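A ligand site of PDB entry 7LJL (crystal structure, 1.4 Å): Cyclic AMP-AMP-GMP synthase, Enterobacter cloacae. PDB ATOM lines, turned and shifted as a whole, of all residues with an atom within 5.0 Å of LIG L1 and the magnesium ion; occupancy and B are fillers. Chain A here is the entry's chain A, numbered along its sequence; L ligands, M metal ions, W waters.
Water W8 bridges the side-chain carboxylate of Asp 197 (2.7 Å) and the guanidinium group of Arg 308 (3.2 Å).
Water W11 lies within hydrogen-bond range of O7 of LIG L1 and N3 of LG2 L2.
Water W2 lies within hydrogen-bond range of a ring nitrogen (ND1) of His 303 and an oxygen (O13) of LIG L1.
Water W3 lies within hydrogen-bond range of O of Asp 122 (2.9 Å), N3 of LIG L1 (3.0 Å) and NE2 of Gln 52 (3.1 Å).
Water W9 lies within hydrogen-bond range of N3 of LIG L1 (3.1 Å) and OD1 of Asp 122 (3.2 Å).
Water W13 lies within hydrogen-bond range of the guanidinium group of Arg 308 (3.3 Å) and an oxygen (O2) of LIG L1 (3.3 Å).
Merely in contact with LIG L1: Val 124 (3.3 Å), His 303 (3.5 Å) and Leu 195 (3.5 Å).
Hydrophobic or aromatic side chains within 4 Å of LIG L1: Val 124, Leu 195 and His 303.
Within 4 Å of LIG L1: Gln 52, Arg 110, Val 124, Leu 195, Asp 197, Arg 198, Arg 205, Thr 206, His 303 and Arg 308.
The nearest printed residue that does not touch LIG L1 is Asp 72 (4.6 Å).
The guanidinium group (NE) of Arg 198 is in salt-bridge range of an oxygen (O8) of LIG L1, 2.9 Å away.
An oxygen (O5) of LIG L1 lies within hydrogen-bond range of the backbone NH (N) of Arg 198 (3.0 Å).
OG1 of Thr 206 is in hydrogen-bond range of N5 of LIG L1 (2.8 Å).
The guanidinium group (NE) of Arg 308 lies within salt-bridge range of an oxygen (O7) of LIG L1 (3.6 Å).
O of Arg 205 lies within hydrogen-bond range of O13 of LIG L1.
The guanidinium group (NH2) of Arg 110 is in salt-bridge range of an oxygen (O5) of LIG L1 (2.7 Å).
The side-chain amide nitrogen (NE2) of Gln 52 lies within hydrogen-bond range of a nitrogen (N4) of LIG L1, 3.0 Å away.
O of Asp 72 lies within hydrogen-bond range of N of Gln 52 (2.9 Å).
NE of Arg 110 sits at hydrogen-bond distance from O of Pro 196, 2.9 Å away.
The backbone NH of Gly 204 lies within hydrogen-bond range of the backbone carbonyl oxygen of Leu 195 (2.8 Å).
The magnesium ion is bound by O1 of LIG L1.
O4 of LIG L1 is bound to the magnesium ion (2.0 Å).
Water W4 binds the magnesium ion.
The magnesium ion is bound by OD1 of Asp 197 (2.1 Å).
Water W8 is bound to the magnesium ion.
Water W1 binds the magnesium ion (2.1 Å).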
ATOM      1  N   GLN A  52     -16.222  -2.979 -18.083  1.00  0.00           N
ATOM      2  CA  GLN A  52     -16.300  -2.384 -19.415  1.00  0.00           C
ATOM      3  C   GLN A  52     -17.745  -2.430 -19.898  1.00  0.00           C
ATOM      4  O   GLN A  52     -18.682  -2.637 -19.134  1.00  0.00           O
ATOM      5  CB  GLN A  52     -15.314  -3.007 -20.416  1.00  0.00           C
ATOM      6  CG  GLN A  52     -15.626  -4.446 -20.719  1.00  0.00           C
ATOM      7  CD  GLN A  52     -15.207  -4.904 -22.125  1.00  0.00           C
ATOM      8  OE1 GLN A  52     -14.725  -4.124 -22.926  1.00  0.00           O
ATOM      9  NE2 GLN A  52     -15.357  -6.170 -22.387  1.00  0.00           N
ATOM     10  N   ASP A  72     -20.090  -6.593 -18.743  1.00  0.00           N
ATOM     11  CA  ASP A  72     -18.877  -6.928 -19.459  1.00  0.00           C
ATOM     12  C   ASP A  72     -17.636  -6.645 -18.632  1.00  0.00           C
ATOM     13  O   ASP A  72     -17.529  -5.592 -17.993  1.00  0.00           O
ATOM     14  CB  ASP A  72     -18.835  -6.131 -20.754  1.00  0.00           C
ATOM     15  CG  ASP A  72     -20.025  -6.420 -21.643  1.00  0.00           C
ATOM     16  OD1 ASP A  72     -20.046  -7.525 -22.233  1.00  0.00           O
ATOM     17  OD2 ASP A  72     -20.940  -5.575 -21.796  1.00  0.00           O
ATOM     18  N   ARG A 110     -16.132 -16.461 -27.638  1.00  0.00           N
ATOM     19  CA  ARG A 110     -15.036 -15.601 -27.265  1.00  0.00           C
ATOM     20  C   ARG A 110     -15.067 -15.149 -25.814  1.00  0.00           C
ATOM     21  O   ARG A 110     -14.180 -14.372 -25.401  1.00  0.00           O
ATOM     22  CB  ARG A 110     -15.020 -14.344 -28.158  1.00  0.00           C
ATOM     23  CG  ARG A 110     -16.253 -13.439 -27.969  1.00  0.00           C
ATOM     24  CD  ARG A 110     -15.886 -11.991 -27.804  1.00  0.00           C
ATOM     25  NE  ARG A 110     -15.059 -11.478 -28.898  1.00  0.00           N
ATOM     26  CZ  ARG A 110     -15.526 -10.924 -30.025  1.00  0.00           C
ATOM     27  NH1 ARG A 110     -16.820 -10.836 -30.261  1.00  0.00           N
ATOM     28  NH2 ARG A 110     -14.671 -10.451 -30.926  1.00  0.00           N
ATOM     29  N   ASP A 122     -19.884 -11.181 -18.322  1.00  0.00           N
ATOM     30  CA  ASP A 122     -19.455 -11.569 -19.675  1.00  0.00           C
ATOM     31  C   ASP A 122     -17.963 -11.244 -19.715  1.00  0.00           C
ATOM     32  O   ASP A 122     -17.577 -10.093 -19.882  1.00  0.00           O
ATOM     33  CB  ASP A 122     -20.263 -10.814 -20.727  1.00  0.00           C
ATOM     34  CG  ASP A 122     -19.875 -11.130 -22.130  1.00  0.00           C
ATOM     35  OD1 ASP A 122     -18.868 -11.813 -22.322  1.00  0.00           O
ATOM     36  OD2 ASP A 122     -20.561 -10.675 -23.081  1.00  0.00           O
ATOM     37  N   VAL A 124     -14.095 -11.452 -20.990  1.00  0.00           N
ATOM     38  CA  VAL A 124     -13.242 -11.653 -22.152  1.00  0.00           C
ATOM     39  C   VAL A 124     -11.794 -11.606 -21.699  1.00  0.00           C
ATOM     40  O   VAL A 124     -11.425 -10.751 -20.898  1.00  0.00           O
ATOM     41  CB  VAL A 124     -13.494 -10.656 -23.287  1.00  0.00           C
ATOM     42  CG1 VAL A 124     -14.901 -10.850 -23.856  1.00  0.00           C
ATOM     43  CG2 VAL A 124     -13.261  -9.218 -22.865  1.00  0.00           C
ATOM     44  N   LEU A 195      -8.122  -9.450 -28.292  1.00  0.00           N
ATOM     45  CA  LEU A 195      -9.140 -10.324 -27.742  1.00  0.00           C
ATOM     46  C   LEU A 195      -9.472 -11.430 -28.748  1.00  0.00           C
ATOM     47  O   LEU A 195      -9.137 -11.346 -29.928  1.00  0.00           O
ATOM     48  CB  LEU A 195     -10.388  -9.520 -27.389  1.00  0.00           C
ATOM     49  CG  LEU A 195     -11.408  -9.319 -28.512  1.00  0.00           C
ATOM     50  CD1 LEU A 195     -12.688  -8.725 -27.918  1.00  0.00           C
ATOM     51  CD2 LEU A 195     -10.866  -8.484 -29.621  1.00  0.00           C
ATOM     52  N   PRO A 196     -10.124 -12.490 -28.323  1.00  0.00           N
ATOM     53  CA  PRO A 196     -10.528 -13.518 -29.292  1.00  0.00           C
ATOM     54  C   PRO A 196     -11.554 -13.000 -30.295  1.00  0.00           C
ATOM     55  O   PRO A 196     -12.483 -12.272 -29.963  1.00  0.00           O
ATOM     56  CB  PRO A 196     -11.148 -14.609 -28.404  1.00  0.00           C
ATOM     57  CG  PRO A 196     -10.667 -14.306 -27.008  1.00  0.00           C
ATOM     58  CD  PRO A 196     -10.579 -12.802 -26.953  1.00  0.00           C
ATOM     59  N   ASP A 197     -11.385 -13.423 -31.546  1.00  0.00           N
ATOM     60  CA  ASP A 197     -12.393 -13.160 -32.576  1.00  0.00           C
ATOM     61  C   ASP A 197     -13.715 -13.820 -32.191  1.00  0.00           C
ATOM     62  O   ASP A 197     -13.759 -14.790 -31.434  1.00  0.00           O
ATOM     63  CB  ASP A 197     -11.885 -13.684 -33.916  1.00  0.00           C
ATOM     64  CG  ASP A 197     -12.873 -13.483 -35.038  1.00  0.00           C
ATOM     65  OD1 ASP A 197     -13.021 -12.332 -35.525  1.00  0.00           O
ATOM     66  OD2 ASP A 197     -13.503 -14.477 -35.441  1.00  0.00           O
ATOM     67  N   ARG A 198     -14.813 -13.283 -32.743  1.00  0.00           N
ATOM     68  CA  ARG A 198     -16.129 -13.850 -32.410  1.00  0.00           C
ATOM     69  C   ARG A 198     -16.212 -15.334 -32.776  1.00  0.00           C
ATOM     70  O   ARG A 198     -16.808 -16.119 -32.038  1.00  0.00           O
ATOM     71  CB  ARG A 198     -17.240 -13.076 -33.129  1.00  0.00           C
ATOM     72  CG  ARG A 198     -18.623 -13.587 -32.749  1.00  0.00           C
ATOM     73  CD  ARG A 198     -19.733 -13.035 -33.643  1.00  0.00           C
ATOM     74  NE  ARG A 198     -19.943 -11.616 -33.387  1.00  0.00           N
ATOM     75  CZ  ARG A 198     -21.083 -10.985 -33.660  1.00  0.00           C
ATOM     76  NH1 ARG A 198     -22.109 -11.652 -34.193  1.00  0.00           N
ATOM     77  NH2 ARG A 198     -21.201  -9.687 -33.416  1.00  0.00           N
ATOM     78  N   GLY A 204      -8.068 -10.582 -32.393  1.00  0.00           N
ATOM     79  CA  GLY A 204      -8.440  -9.327 -32.986  1.00  0.00           C
ATOM     80  C   GLY A 204      -8.104  -8.199 -32.032  1.00  0.00           C
ATOM     81  O   GLY A 204      -7.572  -8.420 -30.956  1.00  0.00           O
ATOM     82  N   ARG A 205      -8.336  -6.976 -32.480  1.00  0.00           N
ATOM     83  CA  ARG A 205      -8.019  -5.802 -31.692  1.00  0.00           C
ATOM     84  C   ARG A 205      -9.280  -5.159 -31.112  1.00  0.00           C
ATOM     85  O   ARG A 205     -10.327  -5.101 -31.771  1.00  0.00           O
ATOM     86  CB  ARG A 205      -7.271  -4.763 -32.526  1.00  0.00           C
ATOM     87  CG  ARG A 205      -5.855  -5.194 -32.864  1.00  0.00           C
ATOM     88  CD  ARG A 205      -5.197  -4.222 -33.837  1.00  0.00           C
ATOM     89  NE  ARG A 205      -5.918  -4.206 -35.085  1.00  0.00           N
ATOM     90  CZ  ARG A 205      -5.651  -3.397 -36.107  1.00  0.00           C
ATOM     91  NH1 ARG A 205      -4.668  -2.515 -36.007  1.00  0.00           N
ATOM     92  NH2 ARG A 205      -6.362  -3.462 -37.218  1.00  0.00           N
ATOM     93  N   THR A 206      -9.173  -4.663 -29.877  1.00  0.00           N
ATOM     94  CA  THR A 206     -10.240  -3.918 -29.210  1.00  0.00           C
ATOM     95  C   THR A 206      -9.615  -2.886 -28.284  1.00  0.00           C
ATOM     96  O   THR A 206      -8.561  -3.104 -27.695  1.00  0.00           O
ATOM     97  CB  THR A 206     -11.146  -4.848 -28.411  1.00  0.00           C
ATOM     98  OG1 THR A 206     -12.235  -4.072 -27.880  1.00  0.00           O
ATOM     99  CG2 THR A 206     -10.404  -5.513 -27.240  1.00  0.00           C
ATOM    100  N   HIS A 207     -10.262  -1.740 -28.148  1.00  0.00           N
ATOM    101  CA  HIS A 207      -9.733  -0.662 -27.299  1.00  0.00           C
ATOM    102  C   HIS A 207     -10.838  -0.120 -26.402  1.00  0.00           C
ATOM    103  O   HIS A 207     -11.275   1.022 -26.565  1.00  0.00           O
ATOM    104  CB  HIS A 207      -9.099   0.443 -28.147  1.00  0.00           C
ATOM    105  CG  HIS A 207      -8.037   1.197 -27.431  1.00  0.00           C
ATOM    106  ND1 HIS A 207      -7.985   1.281 -26.056  1.00  0.00           N
ATOM    107  CD2 HIS A 207      -6.983   1.899 -27.904  1.00  0.00           C
ATOM    108  CE1 HIS A 207      -6.918   1.994 -25.722  1.00  0.00           C
ATOM    109  NE2 HIS A 207      -6.293   2.382 -26.820  1.00  0.00           N
ATOM    110  N   VAL A 300     -10.659   1.347 -32.062  1.00  0.00           N
ATOM    111  CA  VAL A 300      -9.772   0.896 -33.125  1.00  0.00           C
ATOM    112  C   VAL A 300     -10.232   1.580 -34.419  1.00  0.00           C
ATOM    113  O   VAL A 300     -11.202   1.162 -35.055  1.00  0.00           O
ATOM    114  CB  VAL A 300      -9.812  -0.629 -33.259  1.00  0.00           C
ATOM    115  CG1 VAL A 300      -8.853  -1.109 -34.334  1.00  0.00           C
ATOM    116  CG2 VAL A 300      -9.464  -1.305 -31.916  1.00  0.00           C
ATOM    117  N   HIS A 303     -11.423  -0.095 -37.689  1.00  0.00           N
ATOM    118  CA  HIS A 303     -12.573  -0.984 -37.673  1.00  0.00           C
ATOM    119  C   HIS A 303     -13.853  -0.236 -37.995  1.00  0.00           C
ATOM    120  O   HIS A 303     -14.103   0.853 -37.465  1.00  0.00           O
ATOM    121  CB  HIS A 303     -12.722  -1.612 -36.286  1.00  0.00           C
ATOM    122  CG  HIS A 303     -11.745  -2.686 -35.996  1.00  0.00           C
ATOM    123  ND1 HIS A 303     -11.712  -3.348 -34.781  1.00  0.00           N
ATOM    124  CD2 HIS A 303     -10.789  -3.264 -36.769  1.00  0.00           C
ATOM    125  CE1 HIS A 303     -10.764  -4.274 -34.817  1.00  0.00           C
ATOM    126  NE2 HIS A 303     -10.191  -4.237 -36.008  1.00  0.00           N
ATOM    127  N   ARG A 308     -20.928  -5.903 -39.337  1.00  0.00           N
ATOM    128  CA  ARG A 308     -21.874  -7.020 -39.367  1.00  0.00           C
ATOM    129  C   ARG A 308     -23.319  -6.598 -39.616  1.00  0.00           C
ATOM    130  O   ARG A 308     -24.178  -7.466 -39.766  1.00  0.00           O
ATOM    131  CB  ARG A 308     -21.765  -7.862 -38.110  1.00  0.00           C
ATOM    132  CG  ARG A 308     -20.481  -8.660 -38.054  1.00  0.00           C
ATOM    133  CD  ARG A 308     -20.321  -9.432 -36.740  1.00  0.00           C
ATOM    134  NE  ARG A 308     -19.118 -10.242 -36.769  1.00  0.00           N
ATOM    135  CZ  ARG A 308     -19.087 -11.537 -37.086  1.00  0.00           C
ATOM    136  NH1 ARG A 308     -20.194 -12.165 -37.422  1.00  0.00           N
ATOM    137  NH2 ARG A 308     -17.927 -12.192 -37.040  1.00  0.00           N
HETATM  138  P1  LIG L   1     -13.371  -8.477 -36.284  1.00  0.00           P
HETATM  139  O1  LIG L   1     -13.100  -9.819 -36.917  1.00  0.00           O
HETATM  140  O2  LIG L   1     -13.798  -7.453 -37.283  1.00  0.00           O
HETATM  141  O3  LIG L   1     -12.291  -7.990 -35.319  1.00  0.00           O
HETATM  142  P2  LIG L   1     -15.474  -9.938 -34.937  1.00  0.00           P
HETATM  143  O4  LIG L   1     -15.538 -10.932 -36.079  1.00  0.00           O
HETATM  144  O5  LIG L   1     -15.024 -10.474 -33.637  1.00  0.00           O
HETATM  145  O6  LIG L   1     -14.646  -8.648 -35.345  1.00  0.00           O
HETATM  146  P3  LIG L   1     -17.677  -8.604 -33.560  1.00  0.00           P
HETATM  147  O7  LIG L   1     -18.807  -7.804 -34.147  1.00  0.00           O
HETATM  148  O8  LIG L   1     -18.004  -9.674 -32.563  1.00  0.00           O
HETATM  149  O9  LIG L   1     -16.921  -9.282 -34.823  1.00  0.00           O
HETATM  150  O10 LIG L   1     -16.579  -7.659 -32.863  1.00  0.00           O
HETATM  151  C1  LIG L   1     -16.249  -6.449 -33.488  1.00  0.00           C
HETATM  152  C2  LIG L   1     -15.261  -5.710 -32.619  1.00  0.00           C
HETATM  153  O11 LIG L   1     -15.916  -5.409 -31.353  1.00  0.00           O
HETATM  154  C3  LIG L   1     -14.036  -6.501 -32.230  1.00  0.00           C
HETATM  155  O12 LIG L   1     -12.980  -6.327 -33.148  1.00  0.00           O
HETATM  156  C4  LIG L   1     -13.665  -5.890 -30.890  1.00  0.00           C
HETATM  157  O13 LIG L   1     -12.924  -4.673 -31.122  1.00  0.00           O
HETATM  158  C5  LIG L   1     -14.993  -5.487 -30.299  1.00  0.00           C
HETATM  159  N1  LIG L   1     -15.563  -6.432 -29.346  1.00  0.00           N
HETATM  160  C6  LIG L   1     -16.507  -7.375 -29.577  1.00  0.00           C
HETATM  161  N2  LIG L   1     -16.844  -8.044 -28.446  1.00  0.00           N
HETATM  162  C7  LIG L   1     -16.140  -7.446 -27.432  1.00  0.00           C
HETATM  163  C8  LIG L   1     -16.041  -7.619 -26.006  1.00  0.00           C
HETATM  164  N3  LIG L   1     -16.786  -8.548 -25.381  1.00  0.00           N
HETATM  165  N4  LIG L   1     -15.231  -6.804 -25.316  1.00  0.00           N
HETATM  166  C9  LIG L   1     -14.477  -5.869 -25.914  1.00  0.00           C
HETATM  167  N5  LIG L   1     -14.492  -5.657 -27.236  1.00  0.00           N
HETATM  168  C10 LIG L   1     -15.318  -6.407 -28.004  1.00  0.00           C
HETATM  169  P1  LG2 L   2     -25.465  -4.144 -24.107  1.00  0.00           P
HETATM  170  O1  LG2 L   2     -24.686  -5.258 -23.497  1.00  0.00           O
HETATM  171  O2  LG2 L   2     -26.469  -4.482 -25.198  1.00  0.00           O
HETATM  172  O3  LG2 L   2     -26.017  -3.117 -23.111  1.00  0.00           O
HETATM  173  P2  LG2 L   2     -22.781  -3.271 -24.822  1.00  0.00           P
HETATM  174  O4  LG2 L   2     -22.269  -1.974 -25.335  1.00  0.00           O
HETATM  175  O5  LG2 L   2     -22.348  -3.730 -23.459  1.00  0.00           O
HETATM  176  O6  LG2 L   2     -24.371  -3.196 -24.903  1.00  0.00           O
HETATM  177  P3  LG2 L   2     -21.933  -5.929 -25.824  1.00  0.00           P
HETATM  178  O7  LG2 L   2     -22.107  -6.423 -24.424  1.00  0.00           O
HETATM  179  O8  LG2 L   2     -22.602  -6.603 -26.986  1.00  0.00           O
HETATM  180  O9  LG2 L   2     -22.349  -4.372 -25.917  1.00  0.00           O
HETATM  181  O10 LG2 L   2     -20.388  -5.811 -26.171  1.00  0.00           O
HETATM  182  C1  LG2 L   2     -19.429  -5.528 -25.150  1.00  0.00           C
HETATM  183  C2  LG2 L   2     -18.487  -4.450 -25.647  1.00  0.00           C
HETATM  184  O11 LG2 L   2     -17.723  -4.932 -26.778  1.00  0.00           O
HETATM  185  C3  LG2 L   2     -19.127  -3.164 -26.118  1.00  0.00           C
HETATM  186  O12 LG2 L   2     -19.531  -2.288 -25.092  1.00  0.00           O
HETATM  187  C4  LG2 L   2     -17.994  -2.576 -26.970  1.00  0.00           C
HETATM  188  O13 LG2 L   2     -16.978  -2.014 -26.144  1.00  0.00           O
HETATM  189  C5  LG2 L   2     -17.444  -3.815 -27.648  1.00  0.00           C
HETATM  190  N1  LG2 L   2     -18.123  -4.054 -28.927  1.00  0.00           N
HETATM  191  C6  LG2 L   2     -19.061  -4.974 -29.241  1.00  0.00           C
HETATM  192  N2  LG2 L   2     -19.457  -4.878 -30.536  1.00  0.00           N
HETATM  193  C7  LG2 L   2     -18.684  -3.874 -31.077  1.00  0.00           C
HETATM  194  C8  LG2 L   2     -18.540  -3.304 -32.388  1.00  0.00           C
HETATM  195  N3  LG2 L   2     -19.293  -3.702 -33.453  1.00  0.00           N
HETATM  196  N4  LG2 L   2     -17.647  -2.324 -32.511  1.00  0.00           N
HETATM  197  C9  LG2 L   2     -16.870  -1.911 -31.496  1.00  0.00           C
HETATM  198  N5  LG2 L   2     -16.955  -2.368 -30.233  1.00  0.00           N
HETATM  199  C10 LG2 L   2     -17.819  -3.371 -30.011  1.00  0.00           C
HETATM  200 MG    MG M   1     -13.978 -11.561 -37.213  1.00  0.00          MG
HETATM  201  O   HOH W   1     -12.314 -12.334 -38.316  1.00  0.00           O
HETATM  202  O   HOH W   2     -13.426  -2.480 -32.807  1.00  0.00           O
HETATM  203  O   HOH W   3     -17.362  -8.594 -22.402  1.00  0.00           O
HETATM  204  O   HOH W   4     -14.697 -10.856 -38.985  1.00  0.00           O
HETATM  205  O   HOH W   5     -19.531  -8.915 -28.210  1.00  0.00           O
HETATM  206  O   HOH W   6     -18.412  -6.222 -36.367  1.00  0.00           O
HETATM  207  O   HOH W   7     -14.201  -4.985 -37.286  1.00  0.00           O
HETATM  208  O   HOH W   8     -14.973 -13.438 -37.388  1.00  0.00           O
HETATM  209  O   HOH W   9     -18.525 -11.110 -25.404  1.00  0.00           O
HETATM  210  O   HOH W  10     -11.023  -6.747 -38.866  1.00  0.00           O
HETATM  211  O   HOH W  11     -20.925  -6.200 -33.926  1.00  0.00           O
HETATM  212  O   HOH W  12     -11.055  -9.497 -38.896  1.00  0.00           O
HETATM  213  O   HOH W  13     -16.969  -8.105 -37.991  1.00  0.00           O
